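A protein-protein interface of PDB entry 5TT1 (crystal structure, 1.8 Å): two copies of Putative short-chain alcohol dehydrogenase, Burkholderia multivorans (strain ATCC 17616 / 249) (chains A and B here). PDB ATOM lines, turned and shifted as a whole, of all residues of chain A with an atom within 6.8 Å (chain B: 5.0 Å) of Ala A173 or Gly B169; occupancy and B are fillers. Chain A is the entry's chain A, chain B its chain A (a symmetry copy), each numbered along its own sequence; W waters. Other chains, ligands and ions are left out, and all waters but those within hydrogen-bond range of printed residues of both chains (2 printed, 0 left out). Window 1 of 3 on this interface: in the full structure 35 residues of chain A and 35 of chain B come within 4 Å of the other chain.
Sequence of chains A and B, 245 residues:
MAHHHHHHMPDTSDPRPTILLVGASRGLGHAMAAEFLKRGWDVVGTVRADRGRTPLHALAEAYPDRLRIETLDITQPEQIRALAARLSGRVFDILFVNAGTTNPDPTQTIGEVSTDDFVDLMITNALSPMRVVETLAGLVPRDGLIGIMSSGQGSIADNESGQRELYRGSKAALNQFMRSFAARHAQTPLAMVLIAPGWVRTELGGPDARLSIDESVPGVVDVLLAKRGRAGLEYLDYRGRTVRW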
ATOM      1  N   MET A 122     -22.327   5.624   6.816  1.00  0.00           N
ATOM      2  CA  MET A 122     -22.503   5.428   8.256  1.00  0.00           C
ATOM      3  C   MET A 122     -21.271   5.905   9.018  1.00  0.00           C
ATOM      4  O   MET A 122     -21.386   6.481  10.112  1.00  0.00           O
ATOM      5  CB  MET A 122     -22.783   3.958   8.577  1.00  0.00           C
ATOM      6  CG  MET A 122     -24.159   3.458   8.125  1.00  0.00           C
ATOM      7  SD  MET A 122     -25.553   4.461   8.678  1.00  0.00           S
ATOM      8  CE  MET A 122     -25.283   4.502  10.417  1.00  0.00           C
ATOM      9  N   ASN A 125     -21.176   9.926   8.630  1.00  0.00           N
ATOM     10  CA  ASN A 125     -22.303  10.689   9.156  1.00  0.00           C
ATOM     11  C   ASN A 125     -22.661  10.343  10.598  1.00  0.00           C
ATOM     12  O   ASN A 125     -23.331  11.143  11.259  1.00  0.00           O
ATOM     13  CB  ASN A 125     -23.553  10.471   8.285  1.00  0.00           C
ATOM     14  CG  ASN A 125     -23.488  11.205   6.963  1.00  0.00           C
ATOM     15  OD1 ASN A 125     -22.425  11.681   6.539  1.00  0.00           O
ATOM     16  ND2 ASN A 125     -24.632  11.318   6.305  1.00  0.00           N
ATOM     17  N   ALA A 126     -22.272   9.170  11.100  1.00  0.00           N
ATOM     18  CA  ALA A 126     -22.650   8.798  12.461  1.00  0.00           C
ATOM     19  C   ALA A 126     -21.449   8.483  13.340  1.00  0.00           C
ATOM     20  O   ALA A 126     -21.361   8.996  14.463  1.00  0.00           O
ATOM     21  CB  ALA A 126     -23.631   7.605  12.442  1.00  0.00           C
ATOM     22  N   MET A 130     -19.553  11.556  16.021  1.00  0.00           N
ATOM     23  CA  MET A 130     -19.544  11.208  17.433  1.00  0.00           C
ATOM     24  C   MET A 130     -18.124  11.102  17.969  1.00  0.00           C
ATOM     25  O   MET A 130     -17.885  11.431  19.131  1.00  0.00           O
ATOM     26  CB  MET A 130     -20.320   9.913  17.676  1.00  0.00           C
ATOM     27  CG  MET A 130     -21.832  10.115  17.570  1.00  0.00           C
ATOM     28  SD  MET A 130     -22.427  11.484  18.632  1.00  0.00           S
ATOM     29  CE  MET A 130     -21.806  11.029  20.251  1.00  0.00           C
ATOM     30  N   GLY A 154     -33.355  13.063   9.911  1.00  0.00           N
ATOM     31  CA  GLY A 154     -33.016  12.105  10.938  1.00  0.00           C
ATOM     32  C   GLY A 154     -34.136  11.773  11.896  1.00  0.00           C
ATOM     33  O   GLY A 154     -34.036  10.781  12.627  1.00  0.00           O
ATOM     34  N   ILE A 156     -37.225  10.108  13.259  1.00  0.00           N
ATOM     35  CA  ILE A 156     -37.973   8.906  12.907  1.00  0.00           C
ATOM     36  C   ILE A 156     -39.476   9.172  12.975  1.00  0.00           C
ATOM     37  O   ILE A 156     -40.224   8.760  12.084  1.00  0.00           O
ATOM     38  CB  ILE A 156     -37.553   7.720  13.800  1.00  0.00           C
ATOM     39  CG1 ILE A 156     -36.039   7.500  13.711  1.00  0.00           C
ATOM     40  CG2 ILE A 156     -38.288   6.450  13.389  1.00  0.00           C
ATOM     41  CD1 ILE A 156     -35.553   6.173  14.307  1.00  0.00           C
ATOM     42  N   ARG A 168     -31.147   9.279   5.662  1.00  0.00           N
ATOM     43  CA  ARG A 168     -32.037   9.295   6.820  1.00  0.00           C
ATOM     44  C   ARG A 168     -31.561   8.341   7.907  1.00  0.00           C
ATOM     45  O   ARG A 168     -31.559   8.687   9.097  1.00  0.00           O
ATOM     46  CB  ARG A 168     -33.458   8.932   6.400  1.00  0.00           C
ATOM     47  CG  ARG A 168     -34.212   9.957   5.598  1.00  0.00           C
ATOM     48  CD  ARG A 168     -35.635   9.376   5.419  1.00  0.00           C
ATOM     49  NE  ARG A 168     -36.652  10.269   4.879  1.00  0.00           N
ATOM     50  CZ  ARG A 168     -37.279  11.214   5.579  1.00  0.00           C
ATOM     51  NH1 ARG A 168     -36.969  11.417   6.855  1.00  0.00           N
ATOM     52  NH2 ARG A 168     -38.224  11.954   5.002  1.00  0.00           N
ATOM     53  N   GLY A 169     -31.143   7.138   7.521  1.00  0.00           N
ATOM     54  CA  GLY A 169     -30.714   6.176   8.520  1.00  0.00           C
ATOM     55  C   GLY A 169     -29.437   6.611   9.209  1.00  0.00           C
ATOM     56  O   GLY A 169     -29.251   6.359  10.404  1.00  0.00           O
ATOM     57  N   SER A 170     -28.533   7.249   8.456  1.00  0.00           N
ATOM     58  CA  SER A 170     -27.281   7.717   9.050  1.00  0.00           C
ATOM     59  C   SER A 170     -27.551   8.781  10.107  1.00  0.00           C
ATOM     60  O   SER A 170     -26.912   8.804  11.166  1.00  0.00           O
ATOM     61  CB  SER A 170     -26.346   8.244   7.955  1.00  0.00           C
ATOM     62  OG  SER A 170     -26.733   9.521   7.446  1.00  0.00           O
ATOM     63  N   LYS A 171     -28.515   9.660   9.846  1.00  0.00           N
ATOM     64  CA  LYS A 171     -28.798  10.751  10.771  1.00  0.00           C
ATOM     65  C   LYS A 171     -29.629  10.283  11.968  1.00  0.00           C
ATOM     66  O   LYS A 171     -29.500  10.843  13.062  1.00  0.00           O
ATOM     67  CB  LYS A 171     -29.512  11.886  10.022  1.00  0.00           C
ATOM     68  CG  LYS A 171     -28.640  12.661   9.021  1.00  0.00           C
ATOM     69  CD  LYS A 171     -27.602  13.499   9.770  1.00  0.00           C
ATOM     70  CE  LYS A 171     -26.819  14.414   8.848  1.00  0.00           C
ATOM     71  NZ  LYS A 171     -25.771  15.149   9.624  1.00  0.00           N
ATOM     72  N   ALA A 172     -30.488   9.275  11.797  1.00  0.00           N
ATOM     73  CA  ALA A 172     -31.178   8.730  12.962  1.00  0.00           C
ATOM     74  C   ALA A 172     -30.190   8.033  13.896  1.00  0.00           C
ATOM     75  O   ALA A 172     -30.283   8.160  15.120  1.00  0.00           O
ATOM     76  CB  ALA A 172     -32.289   7.777  12.508  1.00  0.00           C
ATOM     77  N   ALA A 173     -29.221   7.303  13.344  1.00  0.00           N
ATOM     78  CA  ALA A 173     -28.190   6.702  14.189  1.00  0.00           C
ATOM     79  C   ALA A 173     -27.387   7.770  14.920  1.00  0.00           C
ATOM     80  O   ALA A 173     -27.110   7.639  16.122  1.00  0.00           O
ATOM     81  CB  ALA A 173     -27.264   5.825  13.344  1.00  0.00           C
ATOM     82  N   LEU A 174     -27.012   8.838  14.213  1.00  0.00           N
ATOM     83  CA  LEU A 174     -26.342   9.961  14.869  1.00  0.00           C
ATOM     84  C   LEU A 174     -27.158  10.479  16.047  1.00  0.00           C
ATOM     85  O   LEU A 174     -26.643  10.603  17.165  1.00  0.00           O
ATOM     86  CB  LEU A 174     -26.083  11.083  13.864  1.00  0.00           C
ATOM     87  CG  LEU A 174     -25.457  12.367  14.437  1.00  0.00           C
ATOM     88  CD1 LEU A 174     -24.091  12.090  15.040  1.00  0.00           C
ATOM     89  CD2 LEU A 174     -25.321  13.417  13.367  1.00  0.00           C
ATOM     90  N   ASN A 175     -28.445  10.771  15.821  1.00  0.00           N
ATOM     91  CA  ASN A 175     -29.261  11.332  16.897  1.00  0.00           C
ATOM     92  C   ASN A 175     -29.335  10.377  18.083  1.00  0.00           C
ATOM     93  O   ASN A 175     -29.277  10.806  19.241  1.00  0.00           O
ATOM     94  CB  ASN A 175     -30.668  11.671  16.398  1.00  0.00           C
ATOM     95  CG  ASN A 175     -30.686  12.839  15.409  1.00  0.00           C
ATOM     96  OD1 ASN A 175     -31.739  13.205  14.889  1.00  0.00           O
ATOM     97  ND2 ASN A 175     -29.532  13.420  15.147  1.00  0.00           N
ATOM     98  N   GLN A 176     -29.440   9.077  17.816  1.00  0.00           N
ATOM     99  CA  GLN A 176     -29.486   8.108  18.908  1.00  0.00           C
ATOM    100  C   GLN A 176     -28.161   8.062  19.658  1.00  0.00           C
ATOM    101  O   GLN A 176     -28.135   8.050  20.897  1.00  0.00           O
ATOM    102  CB  GLN A 176     -29.852   6.722  18.357  1.00  0.00           C
ATOM    103  CG  GLN A 176     -29.979   5.618  19.441  1.00  0.00           C
ATOM    104  CD  GLN A 176     -31.262   5.701  20.255  1.00  0.00           C
ATOM    105  OE1 GLN A 176     -31.586   6.740  20.823  1.00  0.00           O
ATOM    106  NE2 GLN A 176     -31.992   4.593  20.322  1.00  0.00           N
ATOM    107  N   PHE A 177     -27.053   8.015  18.923  1.00  0.00           N
ATOM    108  CA  PHE A 177     -25.741   8.034  19.558  1.00  0.00           C
ATOM    109  C   PHE A 177     -25.600   9.250  20.470  1.00  0.00           C
ATOM    110  O   PHE A 177     -25.109   9.144  21.604  1.00  0.00           O
ATOM    111  CB  PHE A 177     -24.650   8.059  18.493  1.00  0.00           C
ATOM    112  CG  PHE A 177     -24.465   6.766  17.747  1.00  0.00           C
ATOM    113  CD1 PHE A 177     -24.598   5.539  18.388  1.00  0.00           C
ATOM    114  CD2 PHE A 177     -24.114   6.793  16.408  1.00  0.00           C
ATOM    115  CE1 PHE A 177     -24.402   4.366  17.693  1.00  0.00           C
ATOM    116  CE2 PHE A 177     -23.908   5.613  15.695  1.00  0.00           C
ATOM    117  CZ  PHE A 177     -24.047   4.403  16.341  1.00  0.00           C
ATOM    118  N   MET A 178     -26.040  10.411  19.991  1.00  0.00           N
ATOM    119  CA  MET A 178     -25.921  11.622  20.790  1.00  0.00           C
ATOM    120  C   MET A 178     -26.799  11.558  22.036  1.00  0.00           C
ATOM    121  O   MET A 178     -26.397  12.034  23.100  1.00  0.00           O
ATOM    122  CB  MET A 178     -26.260  12.843  19.938  1.00  0.00           C
ATOM    123  CG  MET A 178     -25.846  14.159  20.594  1.00  0.00           C
ATOM    124  SD  MET A 178     -24.068  14.197  20.948  1.00  0.00           S
ATOM    125  CE  MET A 178     -24.002  15.574  22.097  1.00  0.00           C
ATOM    126  N   ARG A 179     -28.000  10.969  21.934  1.00  0.00           N
ATOM    127  CA  ARG A 179     -28.826  10.827  23.129  1.00  0.00           C
ATOM    128  C   ARG A 179     -28.126   9.986  24.189  1.00  0.00           C
ATOM    129  O   ARG A 179     -28.216  10.287  25.383  1.00  0.00           O
ATOM    130  CB  ARG A 179     -30.188  10.217  22.787  1.00  0.00           C
ATOM    131  CG  ARG A 179     -31.141  11.147  22.036  1.00  0.00           C
ATOM    132  CD  ARG A 179     -32.565  10.973  22.562  1.00  0.00           C
ATOM    133  NE  ARG A 179     -32.789  11.687  23.825  1.00  0.00           N
ATOM    134  CZ  ARG A 179     -33.830  11.491  24.628  1.00  0.00           C
ATOM    135  NH1 ARG A 179     -33.941  12.191  25.750  1.00  0.00           N
ATOM    136  NH2 ARG A 179     -34.756  10.588  24.326  1.00  0.00           N
ATOM    137  N   SER A 180     -27.414   8.929  23.780  1.00  0.00           N
ATOM    138  CA  SER A 180     -26.705   8.137  24.781  1.00  0.00           C
ATOM    139  C   SER A 180     -25.571   8.936  25.409  1.00  0.00           C
ATOM    140  O   SER A 180     -25.348   8.858  26.623  1.00  0.00           O
ATOM    141  CB  SER A 180     -26.165   6.849  24.170  1.00  0.00           C
ATOM    142  OG  SER A 180     -27.219   5.972  23.824  1.00  0.00           O
ATOM    143  N   MET B 122     -23.421  -2.472  12.361  1.00  0.00           N
ATOM    144  CA  MET B 122     -24.338  -1.744  11.481  1.00  0.00           C
ATOM    145  C   MET B 122     -24.758  -2.616  10.302  1.00  0.00           C
ATOM    146  O   MET B 122     -25.919  -2.572   9.863  1.00  0.00           O
ATOM    147  CB  MET B 122     -23.697  -0.450  10.975  1.00  0.00           C
ATOM    148  CG  MET B 122     -23.522   0.635  12.044  1.00  0.00           C
ATOM    149  SD  MET B 122     -25.015   1.036  12.973  1.00  0.00           S
ATOM    150  CE  MET B 122     -26.142   1.412  11.672  1.00  0.00           C
ATOM    151  N   GLU B 165     -24.579   1.326  23.719  1.00  0.00           N
ATOM    152  CA  GLU B 165     -24.658   2.471  22.815  1.00  0.00           C
ATOM    153  C   GLU B 165     -24.619   2.057  21.353  1.00  0.00           C
ATOM    154  O   GLU B 165     -25.378   2.594  20.534  1.00  0.00           O
ATOM    155  CB  GLU B 165     -23.545   3.471  23.127  1.00  0.00           C
ATOM    156  CG  GLU B 165     -23.707   4.079  24.503  1.00  0.00           C
ATOM    157  CD  GLU B 165     -22.990   5.401  24.651  1.00  0.00           C
ATOM    158  OE1 GLU B 165     -22.340   5.847  23.675  1.00  0.00           O
ATOM    159  OE2 GLU B 165     -23.082   5.995  25.746  1.00  0.00           O
ATOM    160  N   LEU B 166     -23.729   1.134  20.992  1.00  0.00           N
ATOM    161  CA  LEU B 166     -23.630   0.764  19.585  1.00  0.00           C
ATOM    162  C   LEU B 166     -24.897   0.054  19.129  1.00  0.00           C
ATOM    163  O   LEU B 166     -25.428   0.336  18.039  1.00  0.00           O
ATOM    164  CB  LEU B 166     -22.392  -0.105  19.359  1.00  0.00           C
ATOM    165  CG  LEU B 166     -22.164  -0.524  17.903  1.00  0.00           C
ATOM    166  CD1 LEU B 166     -22.047   0.682  16.973  1.00  0.00           C
ATOM    167  CD2 LEU B 166     -20.946  -1.430  17.788  1.00  0.00           C
ATOM    168  N   TYR B 167     -25.395  -0.858  19.971  1.00  0.00           N
ATOM    169  CA  TYR B 167     -26.628  -1.584  19.688  1.00  0.00           C
ATOM    170  C   TYR B 167     -27.801  -0.629  19.481  1.00  0.00           C
ATOM    171  O   TYR B 167     -28.571  -0.764  18.522  1.00  0.00           O
ATOM    172  CB  TYR B 167     -26.898  -2.560  20.833  1.00  0.00           C
ATOM    173  CG  TYR B 167     -28.135  -3.405  20.628  1.00  0.00           C
ATOM    174  CD1 TYR B 167     -28.091  -4.552  19.845  1.00  0.00           C
ATOM    175  CD2 TYR B 167     -29.341  -3.058  21.220  1.00  0.00           C
ATOM    176  CE1 TYR B 167     -29.219  -5.342  19.658  1.00  0.00           C
ATOM    177  CE2 TYR B 167     -30.479  -3.836  21.037  1.00  0.00           C
ATOM    178  CZ  TYR B 167     -30.408  -4.976  20.255  1.00  0.00           C
ATOM    179  OH  TYR B 167     -31.520  -5.762  20.073  1.00  0.00           O
ATOM    180  N   ARG B 168     -27.940   0.364  20.362  1.00  0.00           N
ATOM    181  CA  ARG B 168     -29.039   1.316  20.224  1.00  0.00           C
ATOM    182  C   ARG B 168     -29.006   2.022  18.876  1.00  0.00           C
ATOM    183  O   ARG B 168     -30.044   2.180  18.218  1.00  0.00           O
ATOM    184  CB  ARG B 168     -28.990   2.346  21.348  1.00  0.00           C
ATOM    185  CG  ARG B 168     -29.358   1.867  22.725  1.00  0.00           C
ATOM    186  CD  ARG B 168     -29.332   3.128  23.622  1.00  0.00           C
ATOM    187  NE  ARG B 168     -29.881   2.997  24.966  1.00  0.00           N
ATOM    188  CZ  ARG B 168     -31.181   2.990  25.255  1.00  0.00           C
ATOM    189  NH1 ARG B 168     -32.083   3.075  24.283  1.00  0.00           N
ATOM    190  NH2 ARG B 168     -31.581   2.904  26.523  1.00  0.00           N
ATOM    191  N   GLY B 169     -27.822   2.446  18.439  1.00  0.00           N
ATOM    192  CA  GLY B 169     -27.738   3.158  17.177  1.00  0.00           C
ATOM    193  C   GLY B 169     -28.068   2.261  16.002  1.00  0.00           C
ATOM    194  O   GLY B 169     -28.660   2.711  15.015  1.00  0.00           O
ATOM    195  N   SER B 170     -27.665   0.987  16.083  1.00  0.00           N
ATOM    196  CA  SER B 170     -27.957   0.053  14.998  1.00  0.00           C
ATOM    197  C   SER B 170     -29.461  -0.148  14.851  1.00  0.00           C
ATOM    198  O   SER B 170     -29.988  -0.226  13.734  1.00  0.00           O
ATOM    199  CB  SER B 170     -27.239  -1.279  15.243  1.00  0.00           C
ATOM    200  OG  SER B 170     -27.847  -2.071  16.264  1.00  0.00           O
ATOM    201  N   LYS B 171     -30.174  -0.211  15.973  1.00  0.00           N
ATOM    202  CA  LYS B 171     -31.609  -0.466  15.929  1.00  0.00           C
ATOM    203  C   LYS B 171     -32.401   0.791  15.565  1.00  0.00           C
ATOM    204  O   LYS B 171     -33.470   0.690  14.954  1.00  0.00           O
ATOM    205  CB  LYS B 171     -32.070  -1.029  17.282  1.00  0.00           C
ATOM    206  CG  LYS B 171     -31.598  -2.459  17.593  1.00  0.00           C
ATOM    207  CD  LYS B 171     -32.308  -3.456  16.676  1.00  0.00           C
ATOM    208  CE  LYS B 171     -32.009  -4.897  17.042  1.00  0.00           C
ATOM    209  NZ  LYS B 171     -32.668  -5.822  16.067  1.00  0.00           N
ATOM    210  N   ALA B 172     -31.916   1.982  15.929  1.00  0.00           N
ATOM    211  CA  ALA B 172     -32.589   3.190  15.464  1.00  0.00           C
ATOM    212  C   ALA B 172     -32.448   3.337  13.950  1.00  0.00           C
ATOM    213  O   ALA B 172     -33.398   3.718  13.261  1.00  0.00           O
ATOM    214  CB  ALA B 172     -32.031   4.412  16.201  1.00  0.00           C
ATOM    215  N   ALA B 173     -31.274   3.024  13.402  1.00  0.00           N
ATOM    216  CA  ALA B 173     -31.118   3.048  11.947  1.00  0.00           C
ATOM    217  C   ALA B 173     -32.044   2.040  11.279  1.00  0.00           C
ATOM    218  O   ALA B 173     -32.689   2.350  10.266  1.00  0.00           O
ATOM    219  CB  ALA B 173     -29.663   2.766  11.570  1.00  0.00           C
HETATM  220  O   HOH W   1     -23.820   6.559  21.697  1.00  0.00           O
HETATM  221  O   HOH W   2     -26.192   5.121  21.607  1.00  0.00           O
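Ala A173 touches one residue of chain B. Of chain A, only Ala A173, Gln A176 and Phe A177 come within 4 Å of Gly B169. Printed residues of chain B within 4 Å of Gln A176: Arg B168 (3.6 Å), Gly B169 (3.96 Å) and Ala B172 (3.8 Å). Printed residues of chain A within 4 Å of Glu B165: Phe A177 and Ser A180. Printed residues of chain B within 4 Å of Ser A180: Glu B165 and Arg B168. Of the printed residues of chain A, Met B122 touches Met A122 (3.4 Å). The nearest residue of chain A that does not touch Gly B169 is Ala A172 (5.6 Å). The nearest printed residue of chain B that does not touch Gln A176 is Glu B165 (5.6 Å).
Printed residues of chain A that touch a printed residue of chain B: Met A122, Ile A156, Gly A169, Ala A173, Gln A176, Phe A177 and Ser A180. Along chain A the printed residues that touch a printed residue of chain B span positions 122 to 180. Of the 10 printed residues of chain B, 6 touch a printed residue of chain A. Among the printed residues, 11 pairs touch across the chains. Among the printed residues, no Asp or Glu carboxylate lies within 4 Å of a Lys or Arg side-chain nitrogen of the other chain.
CD1 of Ile A156 touches O of Ala B172 (3.4 Å). Ala B173 touches Gly A169. Gly B169 touches Ala A173 (O to CB, 3.8 Å). Gln A176 touches Arg B168 (CG to O, 3.6 Å). N of Gly B169 touches CG of Gln A176 (3.96 Å). Gln A176 touches Ala B172. Phe A177 touches Glu B165 (CE1 to O, 3.5 Å). Phe A177 touches Gly B169. Ser A180 touches Glu B165 (CB to CD, 3.5 Å). Arg B168 touches Ser A180 (CD to OG, 3.5 Å).
Met A122 touches its own counterpart, Met B122. Gly A169 touches Ala B173, and with the chains exchanged Ala A173 touches Gly B169. 7 positions are printed for both chains.
Water W1 bridges OE1 of Glu B165 and O of Phe A177. Water W2 lies within hydrogen-bond range of the side-chain hydroxyl of Ser A180 (2.6 Å) and the backbone carbonyl oxygen of Glu B165 (2.9 Å).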
